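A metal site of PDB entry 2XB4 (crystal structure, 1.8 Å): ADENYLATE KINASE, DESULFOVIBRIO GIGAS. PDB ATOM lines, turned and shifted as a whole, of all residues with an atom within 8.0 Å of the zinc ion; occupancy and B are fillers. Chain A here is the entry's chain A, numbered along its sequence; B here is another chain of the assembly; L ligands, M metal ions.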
ATOM      1  N   ILE A 128     -26.721  -9.569  12.202  1.00  0.00           N
ATOM      2  CA  ILE A 128     -27.297  -9.425  13.541  1.00  0.00           C
ATOM      3  C   ILE A 128     -28.532 -10.297  13.614  1.00  0.00           C
ATOM      4  O   ILE A 128     -29.387 -10.257  12.724  1.00  0.00           O
ATOM      5  CB  ILE A 128     -27.767  -7.979  13.783  1.00  0.00           C
ATOM      6  CG1 ILE A 128     -26.657  -6.972  13.521  1.00  0.00           C
ATOM      7  CG2 ILE A 128     -28.317  -7.810  15.259  1.00  0.00           C
ATOM      8  CD1 ILE A 128     -25.268  -7.478  13.929  1.00  0.00           C
ATOM      9  N   CYS A 129     -28.635 -11.088  14.695  1.00  0.00           N
ATOM     10  CA  CYS A 129     -29.819 -11.874  14.961  1.00  0.00           C
ATOM     11  C   CYS A 129     -30.999 -11.039  15.458  1.00  0.00           C
ATOM     12  O   CYS A 129     -30.882 -10.260  16.432  1.00  0.00           O
ATOM     13  CB  CYS A 129     -29.446 -12.962  15.999  1.00  0.00           C
ATOM     14  SG  CYS A 129     -30.862 -14.026  16.548  1.00  0.00           S
ATOM     15  N   LYS A 130     -32.149 -11.235  14.831  1.00  0.00           N
ATOM     16  CA  LYS A 130     -33.391 -10.569  15.225  1.00  0.00           C
ATOM     17  C   LYS A 130     -33.806 -10.899  16.643  1.00  0.00           C
ATOM     18  O   LYS A 130     -34.339 -10.037  17.360  1.00  0.00           O
ATOM     19  CB  LYS A 130     -34.519 -10.927  14.248  1.00  0.00           C
ATOM     20  CG  LYS A 130     -35.597  -9.822  14.199  1.00  0.00           C
ATOM     21  CD  LYS A 130     -36.737 -10.010  13.122  1.00  0.00           C
ATOM     22  CE  LYS A 130     -37.730 -11.169  13.478  1.00  0.00           C
ATOM     23  NZ  LYS A 130     -39.191 -10.728  13.682  1.00  0.00           N
ATOM     24  N   ASN A 131     -33.550 -12.147  17.069  1.00  0.00           N
ATOM     25  CA  ASN A 131     -34.061 -12.591  18.387  1.00  0.00           C
ATOM     26  C   ASN A 131     -33.171 -12.090  19.513  1.00  0.00           C
ATOM     27  O   ASN A 131     -33.663 -11.790  20.622  1.00  0.00           O
ATOM     28  CB  ASN A 131     -34.119 -14.134  18.499  1.00  0.00           C
ATOM     29  CG  ASN A 131     -35.131 -14.777  17.549  1.00  0.00           C
ATOM     30  OD1 ASN A 131     -36.087 -14.156  17.102  1.00  0.00           O
ATOM     31  ND2 ASN A 131     -34.918 -16.050  17.254  1.00  0.00           N
ATOM     32  N   ASN A 132     -31.856 -12.089  19.268  1.00  0.00           N
ATOM     33  CA  ASN A 132     -30.950 -11.619  20.333  1.00  0.00           C
ATOM     34  C   ASN A 132     -29.675 -11.058  19.710  1.00  0.00           C
ATOM     35  O   ASN A 132     -28.892 -11.816  19.116  1.00  0.00           O
ATOM     36  CB  ASN A 132     -30.601 -12.811  21.252  1.00  0.00           C
ATOM     37  CG  ASN A 132     -29.774 -12.381  22.510  1.00  0.00           C
ATOM     38  OD1 ASN A 132     -29.016 -11.423  22.468  1.00  0.00           O
ATOM     39  ND2 ASN A 132     -29.901 -13.145  23.589  1.00  0.00           N
ATOM     40  N   PRO A 133     -29.455  -9.739  19.830  1.00  0.00           N
ATOM     41  CA  PRO A 133     -28.325  -9.127  19.067  1.00  0.00           C
ATOM     42  C   PRO A 133     -26.948  -9.550  19.637  1.00  0.00           C
ATOM     43  O   PRO A 133     -25.956  -9.347  18.976  1.00  0.00           O
ATOM     44  CB  PRO A 133     -28.575  -7.612  19.274  1.00  0.00           C
ATOM     45  CG  PRO A 133     -29.248  -7.512  20.685  1.00  0.00           C
ATOM     46  CD  PRO A 133     -30.172  -8.778  20.673  1.00  0.00           C
ATOM     47  N   ASN A 134     -26.917 -10.223  20.772  1.00  0.00           N
ATOM     48  CA  ASN A 134     -25.645 -10.711  21.398  1.00  0.00           C
ATOM     49  C   ASN A 134     -25.103 -11.883  20.591  1.00  0.00           C
ATOM     50  O   ASN A 134     -23.882 -12.138  20.700  1.00  0.00           O
ATOM     51  CB  ASN A 134     -25.806 -11.271  22.847  1.00  0.00           C
ATOM     52  CG  ASN A 134     -26.295 -10.215  23.907  1.00  0.00           C
ATOM     53  OD1 ASN A 134     -26.219  -8.990  23.690  1.00  0.00           O
ATOM     54  ND2 ASN A 134     -26.725 -10.716  25.097  1.00  0.00           N
ATOM     55  N   HIS A 135     -25.942 -12.607  19.826  1.00  0.00           N
ATOM     56  CA  HIS A 135     -25.524 -13.917  19.169  1.00  0.00           C
ATOM     57  C   HIS A 135     -24.525 -13.671  18.012  1.00  0.00           C
ATOM     58  O   HIS A 135     -24.937 -13.160  17.006  1.00  0.00           O
ATOM     59  CB  HIS A 135     -26.758 -14.671  18.578  1.00  0.00           C
ATOM     60  CG  HIS A 135     -27.711 -15.192  19.632  1.00  0.00           C
ATOM     61  ND1 HIS A 135     -28.956 -15.702  19.316  1.00  0.00           N
ATOM     62  CD2 HIS A 135     -27.566 -15.353  20.973  1.00  0.00           C
ATOM     63  CE1 HIS A 135     -29.578 -16.074  20.436  1.00  0.00           C
ATOM     64  NE2 HIS A 135     -28.744 -15.897  21.448  1.00  0.00           N
ATOM     65  N   PRO A 136     -23.227 -14.047  18.165  1.00  0.00           N
ATOM     66  CA  PRO A 136     -22.276 -13.612  17.093  1.00  0.00           C
ATOM     67  C   PRO A 136     -22.440 -14.401  15.799  1.00  0.00           C
ATOM     68  O   PRO A 136     -22.480 -15.643  15.819  1.00  0.00           O
ATOM     69  CB  PRO A 136     -20.859 -13.841  17.740  1.00  0.00           C
ATOM     70  CG  PRO A 136     -21.096 -13.847  19.235  1.00  0.00           C
ATOM     71  CD  PRO A 136     -22.517 -14.584  19.339  1.00  0.00           C
ATOM     72  N   ASN A 137     -22.577 -13.698  14.668  1.00  0.00           N
ATOM     73  CA  ASN A 137     -22.654 -14.326  13.331  1.00  0.00           C
ATOM     74  C   ASN A 137     -21.826 -13.471  12.391  1.00  0.00           C
ATOM     75  O   ASN A 137     -21.965 -12.253  12.417  1.00  0.00           O
ATOM     76  CB  ASN A 137     -24.090 -14.366  12.758  1.00  0.00           C
ATOM     77  CG  ASN A 137     -25.038 -15.367  13.552  1.00  0.00           C
ATOM     78  OD1 ASN A 137     -25.661 -14.991  14.601  1.00  0.00           O
ATOM     79  ND2 ASN A 137     -25.173 -16.571  13.076  1.00  0.00           N
ATOM     80  N   VAL A 150     -29.589 -18.176   8.545  1.00  0.00           N
ATOM     81  CA  VAL A 150     -30.086 -17.912   9.921  1.00  0.00           C
ATOM     82  C   VAL A 150     -29.064 -17.984  11.017  1.00  0.00           C
ATOM     83  O   VAL A 150     -27.932 -18.505  10.849  1.00  0.00           O
ATOM     84  CB  VAL A 150     -31.361 -18.812  10.316  1.00  0.00           C
ATOM     85  CG1 VAL A 150     -32.493 -18.559   9.315  1.00  0.00           C
ATOM     86  CG2 VAL A 150     -31.022 -20.318  10.325  1.00  0.00           C
ATOM     87  N   CYS A 151     -29.449 -17.429  12.179  1.00  0.00           N
ATOM     88  CA  CYS A 151     -28.534 -17.366  13.320  1.00  0.00           C
ATOM     89  C   CYS A 151     -28.001 -18.745  13.725  1.00  0.00           C
ATOM     90  O   CYS A 151     -28.810 -19.665  13.883  1.00  0.00           O
ATOM     91  CB  CYS A 151     -29.281 -16.721  14.533  1.00  0.00           C
ATOM     92  SG  CYS A 151     -28.196 -16.652  15.985  1.00  0.00           S
ATOM     93  N   ARG A 152     -26.673 -18.913  13.879  1.00  0.00           N
ATOM     94  CA  ARG A 152     -26.055 -20.204  14.217  1.00  0.00           C
ATOM     95  C   ARG A 152     -26.313 -20.594  15.673  1.00  0.00           C
ATOM     96  O   ARG A 152     -26.059 -21.731  16.063  1.00  0.00           O
ATOM     97  CB  ARG A 152     -24.539 -20.101  14.020  1.00  0.00           C
ATOM     98  CG  ARG A 152     -23.923 -19.026  15.016  1.00  0.00           C
ATOM     99  CD  ARG A 152     -22.444 -18.804  14.773  1.00  0.00           C
ATOM    100  NE  ARG A 152     -21.762 -20.085  14.600  1.00  0.00           N
ATOM    101  CZ  ARG A 152     -21.287 -20.773  15.623  1.00  0.00           C
ATOM    102  NH1 ARG A 152     -21.451 -20.246  16.864  1.00  0.00           N
ATOM    103  NH2 ARG A 152     -20.667 -21.968  15.408  1.00  0.00           N
ATOM    104  N   VAL A 153     -26.782 -19.657  16.495  1.00  0.00           N
ATOM    105  CA  VAL A 153     -27.059 -19.963  17.934  1.00  0.00           C
ATOM    106  C   VAL A 153     -28.499 -20.392  18.085  1.00  0.00           C
ATOM    107  O   VAL A 153     -28.772 -21.383  18.760  1.00  0.00           O
ATOM    108  CB  VAL A 153     -26.866 -18.691  18.829  1.00  0.00           C
ATOM    109  CG1 VAL A 153     -27.148 -19.025  20.329  1.00  0.00           C
ATOM    110  CG2 VAL A 153     -25.454 -18.125  18.725  1.00  0.00           C
ATOM    111  N   CYS A 154     -29.448 -19.654  17.502  1.00  0.00           N
ATOM    112  CA  CYS A 154     -30.866 -19.903  17.817  1.00  0.00           C
ATOM    113  C   CYS A 154     -31.778 -20.074  16.611  1.00  0.00           C
ATOM    114  O   CYS A 154     -32.977 -20.370  16.790  1.00  0.00           O
ATOM    115  CB  CYS A 154     -31.449 -18.796  18.726  1.00  0.00           C
ATOM    116  SG  CYS A 154     -31.713 -17.213  17.749  1.00  0.00           S
ATOM    117  N   GLY A 155     -31.254 -19.906  15.401  1.00  0.00           N
ATOM    118  CA  GLY A 155     -32.040 -20.065  14.167  1.00  0.00           C
ATOM    119  C   GLY A 155     -32.869 -18.837  13.830  1.00  0.00           C
ATOM    120  O   GLY A 155     -33.621 -18.835  12.863  1.00  0.00           O
ATOM    121  N   GLY A 156     -32.687 -17.743  14.553  1.00  0.00           N
ATOM    122  CA  GLY A 156     -33.410 -16.499  14.224  1.00  0.00           C
ATOM    123  C   GLY A 156     -32.964 -15.890  12.896  1.00  0.00           C
ATOM    124  O   GLY A 156     -31.882 -16.159  12.377  1.00  0.00           O
ATOM    125  N   ALA A 157     -33.812 -15.026  12.372  1.00  0.00           N
ATOM    126  CA  ALA A 157     -33.477 -14.280  11.162  1.00  0.00           C
ATOM    127  C   ALA A 157     -32.265 -13.394  11.356  1.00  0.00           C
ATOM    128  O   ALA A 157     -32.025 -12.866  12.468  1.00  0.00           O
ATOM    129  CB  ALA A 157     -34.704 -13.441  10.655  1.00  0.00           C
ATOM    130  N   LEU A 158     -31.513 -13.187  10.255  1.00  0.00           N
ATOM    131  CA  LEU A 158     -30.249 -12.370  10.301  1.00  0.00           C
ATOM    132  C   LEU A 158     -30.442 -11.130   9.448  1.00  0.00           C
ATOM    133  O   LEU A 158     -31.095 -11.177   8.397  1.00  0.00           O
ATOM    134  CB  LEU A 158     -29.041 -13.187   9.734  1.00  0.00           C
ATOM    135  CG  LEU A 158     -28.545 -14.232  10.725  1.00  0.00           C
ATOM    136  CD1 LEU A 158     -27.416 -15.046  10.028  1.00  0.00           C
ATOM    137  CD2 LEU A 158     -28.106 -13.653  12.101  1.00  0.00           C
ATOM    138  N   GLY B  14     -32.688 -18.944  23.297  1.00  0.00           N
ATOM    139  CA  GLY B  14     -31.793 -19.476  22.224  1.00  0.00           C
ATOM    140  C   GLY B  14     -30.402 -19.747  22.768  1.00  0.00           C
ATOM    141  O   GLY B  14     -29.769 -20.787  22.500  1.00  0.00           O
ATOM    142  N   THR B  15     -29.906 -18.815  23.555  1.00  0.00           N
ATOM    143  CA  THR B  15     -28.630 -18.959  24.195  1.00  0.00           C
ATOM    144  C   THR B  15     -28.534 -20.208  25.040  1.00  0.00           C
ATOM    145  O   THR B  15     -27.554 -20.954  24.955  1.00  0.00           O
ATOM    146  CB  THR B  15     -28.303 -17.731  25.046  1.00  0.00           C
ATOM    147  OG1 THR B  15     -28.357 -16.590  24.206  1.00  0.00           O
ATOM    148  CG2 THR B  15     -26.862 -17.847  25.606  1.00  0.00           C
HETATM  149  O1  LIG L   1     -34.112 -12.803  24.786  1.00  0.00           O
HETATM  150  O2  LIG L   1     -32.697 -14.262  23.788  1.00  0.00           O
HETATM  151  C1  LIG L   1     -33.806 -13.692  23.953  1.00  0.00           C
HETATM  152  C2  LIG L   1     -35.041 -14.184  23.331  1.00  0.00           C
HETATM  153  O3  LIG L   1     -35.921 -13.279  22.693  1.00  0.00           O
HETATM  154  C3  LIG L   1     -35.206 -15.656  23.174  1.00  0.00           C
HETATM  155  O4  LIG L   1     -35.805 -15.682  24.493  1.00  0.00           O
HETATM  156  C4  LIG L   1     -36.225 -16.031  22.187  1.00  0.00           C
HETATM  157  O5  LIG L   1     -35.841 -16.175  21.013  1.00  0.00           O
HETATM  158  O6  LIG L   1     -37.378 -16.192  22.579  1.00  0.00           O
HETATM  159 ZN    ZN M   1     -29.810 -15.866  17.486  1.00  0.00          ZN
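Four residues have an atom within 4 Å of the zinc ion: Cys 129, His 135, Cys 151 and Cys 154. The nearest printed residue that does not touch the zinc ion is Val 153 (4.3 Å).
The backbone carbonyl oxygen (O) of His 135 sits close to the side-chain amide oxygen (OD1) of Asn 137 (3.1 Å). The side-chain sulfur of Cys 151 lies close to the side-chain amide oxygen of Asn 137, 3.3 Å away. A ring nitrogen (NE2) of His 135 sits at hydrogen-bond distance from the side-chain hydroxyl (OG1) of Thr 15 of chain B, at 2.9 Å. SG of Cys 129 sits close to N of Asn 132, at 3.5 Å. The side-chain sulfur (SG) of Cys 154 sits close to the backbone NH (N) of Gly 156, 3.4 Å away. The side-chain sulfur (SG) of Cys 154 lies close to the side-chain amide nitrogen (ND2) of Asn 131 (3.4 Å). N of Cys 151 is in hydrogen-bond range of O of Gly 156. SG of Cys 129 sits close to N of Asn 131.
The side-chain amide nitrogen of Asn 132 lies within hydrogen-bond range of an oxygen (O2) of the ligand (3.0 Å). O of Asn 131 sits at hydrogen-bond distance from O3 of the ligand, at 3.4 Å.
The zinc ion is bound by ND1 of His 135 (2.0 Å). The side-chain sulfur (SG) of Cys 129 is bound to the zinc ion (2.3 Å). SG of Cys 151 binds the zinc ion. The zinc ion is bound by SG of Cys 154, at 2.3 Å.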
